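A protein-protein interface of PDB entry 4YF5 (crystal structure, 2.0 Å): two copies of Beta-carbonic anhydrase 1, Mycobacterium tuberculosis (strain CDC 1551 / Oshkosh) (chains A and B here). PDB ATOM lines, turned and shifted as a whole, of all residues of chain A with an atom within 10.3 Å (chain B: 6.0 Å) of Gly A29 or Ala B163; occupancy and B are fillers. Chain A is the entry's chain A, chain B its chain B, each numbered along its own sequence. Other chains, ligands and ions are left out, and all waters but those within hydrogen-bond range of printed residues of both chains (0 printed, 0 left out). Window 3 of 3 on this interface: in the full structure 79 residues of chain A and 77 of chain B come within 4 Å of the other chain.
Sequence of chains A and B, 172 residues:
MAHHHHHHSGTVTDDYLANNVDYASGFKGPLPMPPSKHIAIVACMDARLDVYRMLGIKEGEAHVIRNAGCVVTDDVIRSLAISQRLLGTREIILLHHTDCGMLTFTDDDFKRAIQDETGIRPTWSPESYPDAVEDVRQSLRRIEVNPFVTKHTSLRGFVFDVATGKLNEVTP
N of Thr B164 lies within hydrogen-bond range of OD1 of Asp B161 (3.5 Å).
The backbone NH (N) of Val B162 lies within hydrogen-bond range of the side-chain hydroxyl (OG1) of Thr B98 (2.9 Å).
The side-chain hydroxyl (OH) of Tyr A23 is in hydrogen-bond range of the side-chain carboxylate (OE2) of Glu A59.
The backbone NH of Ala B163 is in hydrogen-bond range of the side-chain carboxylate of Asp B161.
Among the printed residues, merely in contact across the chains: Pro A30 with Val B162 (3.2 Å), Phe A27 with Thr B164 (3.3 Å), Phe A27 with Val B162 (3.4 Å), Phe A27 with Gly B165 (3.5 Å), Phe A27 with Ala B163 (3.5 Å), Ala A24 with Thr B164 (3.6 Å), Tyr A23 with Gly B165 (3.7 Å), Gly A29 with Ala B163 (3.7 Å), Ala A24 with Gly B165 (3.9 Å) and Pro A30 with Ala B163 (3.95 Å).
Of chain B, only Ala B163 comes within 4 Å of Gly A29.
Ala B163 touches just these residues of chain A: Phe A27 (3.5 Å), Gly A29 (3.7 Å) and Pro A30 (3.95 Å).
No residue of chain A comes within 4 Å of Asp B161.
Of chain A, only Phe A27 (3.4 Å) and Pro A30 (3.2 Å) come within 4 Å of Val B162.
Of chain A, only Ala A24 and Phe A27 come within 4 Å of Thr B164.
Printed residues of chain B within 4 Å of Ala A24: Thr B164 (3.6 Å) and Gly B165 (3.9 Å).
Printed residues of chain B within 4 Å of Tyr A23: Gly B165.
Printed residues of chain B within 4 Å of Pro A30: Val B162 and Ala B163.
Of the printed residues of chain B, Phe A27 touches Val B162, Ala B163, Thr B164 and Gly B165.
The nearest residue of chain B that does not touch Gly A29 is Val B162 (4.1 Å).
Printed residues of chain A that touch a printed residue of chain B: Tyr A23, Ala A24, Phe A27, Gly A29 and Pro A30.
Of the 6 printed residues of chain B, 4 touch a printed residue of chain A.
Among the printed residues, 10 pairs touch across the chains.
Among the printed residues, no Asp or Glu carboxylate lies within 4 Å of a Lys or Arg side-chain nitrogen of the other chain.
No position is printed for both chains.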
ATOM      1  N   TYR A  23     -13.439  30.725 -25.753  1.00  0.00           N
ATOM      2  CA  TYR A  23     -14.750  30.111 -25.904  1.00  0.00           C
ATOM      3  C   TYR A  23     -15.437  30.034 -24.554  1.00  0.00           C
ATOM      4  O   TYR A  23     -16.636  30.296 -24.434  1.00  0.00           O
ATOM      5  CB  TYR A  23     -14.641  28.713 -26.513  1.00  0.00           C
ATOM      6  CG  TYR A  23     -15.947  27.956 -26.500  1.00  0.00           C
ATOM      7  CD1 TYR A  23     -16.914  28.160 -27.493  1.00  0.00           C
ATOM      8  CD2 TYR A  23     -16.224  27.041 -25.497  1.00  0.00           C
ATOM      9  CE1 TYR A  23     -18.124  27.453 -27.473  1.00  0.00           C
ATOM     10  CE2 TYR A  23     -17.408  26.344 -25.469  1.00  0.00           C
ATOM     11  CZ  TYR A  23     -18.355  26.549 -26.455  1.00  0.00           C
ATOM     12  OH  TYR A  23     -19.539  25.841 -26.394  1.00  0.00           O
ATOM     13  N   ALA A  24     -14.659  29.679 -23.540  1.00  0.00           N
ATOM     14  CA  ALA A  24     -15.212  29.430 -22.220  1.00  0.00           C
ATOM     15  C   ALA A  24     -15.801  30.718 -21.646  1.00  0.00           C
ATOM     16  O   ALA A  24     -16.899  30.712 -21.086  1.00  0.00           O
ATOM     17  CB  ALA A  24     -14.150  28.857 -21.307  1.00  0.00           C
ATOM     18  N   SER A  25     -15.088  31.827 -21.835  1.00  0.00           N
ATOM     19  CA  SER A  25     -15.490  33.118 -21.274  1.00  0.00           C
ATOM     20  C   SER A  25     -16.865  33.598 -21.747  1.00  0.00           C
ATOM     21  O   SER A  25     -17.579  34.269 -21.005  1.00  0.00           O
ATOM     22  CB  SER A  25     -14.442  34.177 -21.606  1.00  0.00           C
ATOM     23  OG  SER A  25     -14.410  34.432 -22.997  1.00  0.00           O
ATOM     24  N   GLY A  26     -17.237  33.261 -22.978  1.00  0.00           N
ATOM     25  CA  GLY A  26     -18.543  33.633 -23.496  1.00  0.00           C
ATOM     26  C   GLY A  26     -19.537  32.487 -23.569  1.00  0.00           C
ATOM     27  O   GLY A  26     -20.500  32.530 -24.337  1.00  0.00           O
ATOM     28  N   PHE A  27     -19.319  31.459 -22.761  1.00  0.00           N
ATOM     29  CA  PHE A  27     -20.146  30.265 -22.843  1.00  0.00           C
ATOM     30  C   PHE A  27     -21.436  30.396 -22.048  1.00  0.00           C
ATOM     31  O   PHE A  27     -21.438  30.891 -20.918  1.00  0.00           O
ATOM     32  CB  PHE A  27     -19.367  29.046 -22.355  1.00  0.00           C
ATOM     33  CG  PHE A  27     -20.180  27.785 -22.314  1.00  0.00           C
ATOM     34  CD1 PHE A  27     -20.460  27.085 -23.477  1.00  0.00           C
ATOM     35  CD2 PHE A  27     -20.660  27.294 -21.108  1.00  0.00           C
ATOM     36  CE1 PHE A  27     -21.210  25.926 -23.437  1.00  0.00           C
ATOM     37  CE2 PHE A  27     -21.398  26.141 -21.057  1.00  0.00           C
ATOM     38  CZ  PHE A  27     -21.681  25.451 -22.227  1.00  0.00           C
ATOM     39  N   LYS A  28     -22.530  29.935 -22.652  1.00  0.00           N
ATOM     40  CA  LYS A  28     -23.817  29.852 -21.971  1.00  0.00           C
ATOM     41  C   LYS A  28     -24.218  28.385 -21.814  1.00  0.00           C
ATOM     42  O   LYS A  28     -24.163  27.613 -22.777  1.00  0.00           O
ATOM     43  CB  LYS A  28     -24.892  30.627 -22.743  1.00  0.00           C
ATOM     44  CG  LYS A  28     -26.077  31.079 -21.888  1.00  0.00           C
ATOM     45  CD  LYS A  28     -25.670  32.192 -20.922  1.00  0.00           C
ATOM     46  CE  LYS A  28     -26.826  32.628 -20.031  1.00  0.00           C
ATOM     47  NZ  LYS A  28     -27.328  31.512 -19.183  1.00  0.00           N
ATOM     48  N   GLY A  29     -24.620  28.000 -20.607  1.00  0.00           N
ATOM     49  CA  GLY A  29     -24.904  26.604 -20.309  1.00  0.00           C
ATOM     50  C   GLY A  29     -25.126  26.410 -18.826  1.00  0.00           C
ATOM     51  O   GLY A  29     -24.923  27.347 -18.056  1.00  0.00           O
ATOM     52  N   PRO A  30     -25.517  25.191 -18.408  1.00  0.00           N
ATOM     53  CA  PRO A  30     -25.661  23.985 -19.225  1.00  0.00           C
ATOM     54  C   PRO A  30     -27.015  23.835 -19.920  1.00  0.00           C
ATOM     55  O   PRO A  30     -28.014  24.417 -19.496  1.00  0.00           O
ATOM     56  CB  PRO A  30     -25.473  22.866 -18.201  1.00  0.00           C
ATOM     57  CG  PRO A  30     -26.071  23.424 -16.967  1.00  0.00           C
ATOM     58  CD  PRO A  30     -25.781  24.909 -16.986  1.00  0.00           C
ATOM     59  N   LEU A  31     -27.028  23.044 -20.988  1.00  0.00           N
ATOM     60  CA  LEU A  31     -28.247  22.725 -21.712  1.00  0.00           C
ATOM     61  C   LEU A  31     -28.674  21.311 -21.370  1.00  0.00           C
ATOM     62  O   LEU A  31     -27.855  20.517 -20.904  1.00  0.00           O
ATOM     63  CB  LEU A  31     -28.032  22.875 -23.213  1.00  0.00           C
ATOM     64  CG  LEU A  31     -27.593  24.284 -23.597  1.00  0.00           C
ATOM     65  CD1 LEU A  31     -27.481  24.416 -25.100  1.00  0.00           C
ATOM     66  CD2 LEU A  31     -28.572  25.296 -23.042  1.00  0.00           C
ATOM     67  N   PRO A  32     -29.960  20.987 -21.582  1.00  0.00           N
ATOM     68  CA  PRO A  32     -30.367  19.600 -21.340  1.00  0.00           C
ATOM     69  C   PRO A  32     -29.651  18.643 -22.296  1.00  0.00           C
ATOM     70  O   PRO A  32     -29.298  19.037 -23.413  1.00  0.00           O
ATOM     71  CB  PRO A  32     -31.877  19.614 -21.608  1.00  0.00           C
ATOM     72  CG  PRO A  32     -32.272  21.058 -21.584  1.00  0.00           C
ATOM     73  CD  PRO A  32     -31.080  21.819 -22.054  1.00  0.00           C
ATOM     74  N   GLU A  59     -25.959  24.988 -30.410  1.00  0.00           N
ATOM     75  CA  GLU A  59     -25.636  24.056 -29.337  1.00  0.00           C
ATOM     76  C   GLU A  59     -26.906  23.502 -28.705  1.00  0.00           C
ATOM     77  O   GLU A  59     -27.848  24.246 -28.442  1.00  0.00           O
ATOM     78  CB  GLU A  59     -24.771  24.731 -28.266  1.00  0.00           C
ATOM     79  CG  GLU A  59     -23.412  25.190 -28.754  1.00  0.00           C
ATOM     80  CD  GLU A  59     -22.644  25.928 -27.686  1.00  0.00           C
ATOM     81  OE1 GLU A  59     -23.031  25.811 -26.507  1.00  0.00           O
ATOM     82  OE2 GLU A  59     -21.664  26.627 -28.020  1.00  0.00           O
ATOM     83  N   GLY A  60     -26.928  22.194 -28.472  1.00  0.00           N
ATOM     84  CA  GLY A  60     -28.050  21.568 -27.803  1.00  0.00           C
ATOM     85  C   GLY A  60     -29.135  21.028 -28.725  1.00  0.00           C
ATOM     86  O   GLY A  60     -30.090  20.411 -28.269  1.00  0.00           O
ATOM     87  N   THR B  98     -18.620  16.151 -18.992  1.00  0.00           N
ATOM     88  CA  THR B  98     -19.300  15.994 -17.712  1.00  0.00           C
ATOM     89  C   THR B  98     -20.744  15.589 -17.972  1.00  0.00           C
ATOM     90  O   THR B  98     -21.273  15.853 -19.053  1.00  0.00           O
ATOM     91  CB  THR B  98     -19.269  17.299 -16.876  1.00  0.00           C
ATOM     92  OG1 THR B  98     -19.787  18.382 -17.661  1.00  0.00           O
ATOM     93  CG2 THR B  98     -17.837  17.639 -16.421  1.00  0.00           C
ATOM     94  N   ASP B 161     -16.564  20.473 -19.672  1.00  0.00           N
ATOM     95  CA  ASP B 161     -17.602  20.756 -18.683  1.00  0.00           C
ATOM     96  C   ASP B 161     -18.804  21.409 -19.359  1.00  0.00           C
ATOM     97  O   ASP B 161     -18.679  22.527 -19.860  1.00  0.00           O
ATOM     98  CB  ASP B 161     -17.036  21.677 -17.577  1.00  0.00           C
ATOM     99  CG  ASP B 161     -17.999  21.883 -16.413  1.00  0.00           C
ATOM    100  OD1 ASP B 161     -19.236  21.836 -16.605  1.00  0.00           O
ATOM    101  OD2 ASP B 161     -17.512  22.098 -15.282  1.00  0.00           O
ATOM    102  N   VAL B 162     -19.966  20.748 -19.349  1.00  0.00           N
ATOM    103  CA  VAL B 162     -21.129  21.285 -20.070  1.00  0.00           C
ATOM    104  C   VAL B 162     -21.743  22.504 -19.377  1.00  0.00           C
ATOM    105  O   VAL B 162     -22.610  23.173 -19.941  1.00  0.00           O
ATOM    106  CB  VAL B 162     -22.240  20.220 -20.276  1.00  0.00           C
ATOM    107  CG1 VAL B 162     -21.724  19.089 -21.123  1.00  0.00           C
ATOM    108  CG2 VAL B 162     -22.766  19.710 -18.947  1.00  0.00           C
ATOM    109  N   ALA B 163     -21.272  22.808 -18.171  1.00  0.00           N
ATOM    110  CA  ALA B 163     -21.759  23.971 -17.434  1.00  0.00           C
ATOM    111  C   ALA B 163     -20.892  25.222 -17.638  1.00  0.00           C
ATOM    112  O   ALA B 163     -21.390  26.345 -17.538  1.00  0.00           O
ATOM    113  CB  ALA B 163     -21.852  23.649 -15.960  1.00  0.00           C
ATOM    114  N   THR B 164     -19.604  25.040 -17.925  1.00  0.00           N
ATOM    115  CA  THR B 164     -18.701  26.183 -18.022  1.00  0.00           C
ATOM    116  C   THR B 164     -18.062  26.360 -19.392  1.00  0.00           C
ATOM    117  O   THR B 164     -17.658  27.478 -19.763  1.00  0.00           O
ATOM    118  CB  THR B 164     -17.578  26.071 -16.999  1.00  0.00           C
ATOM    119  OG1 THR B 164     -16.796  24.907 -17.298  1.00  0.00           O
ATOM    120  CG2 THR B 164     -18.162  25.951 -15.596  1.00  0.00           C
ATOM    121  N   GLY B 165     -17.971  25.265 -20.146  1.00  0.00           N
ATOM    122  CA  GLY B 165     -17.357  25.303 -21.463  1.00  0.00           C
ATOM    123  C   GLY B 165     -15.855  25.082 -21.432  1.00  0.00           C
ATOM    124  O   GLY B 165     -15.166  25.219 -22.454  1.00  0.00           O
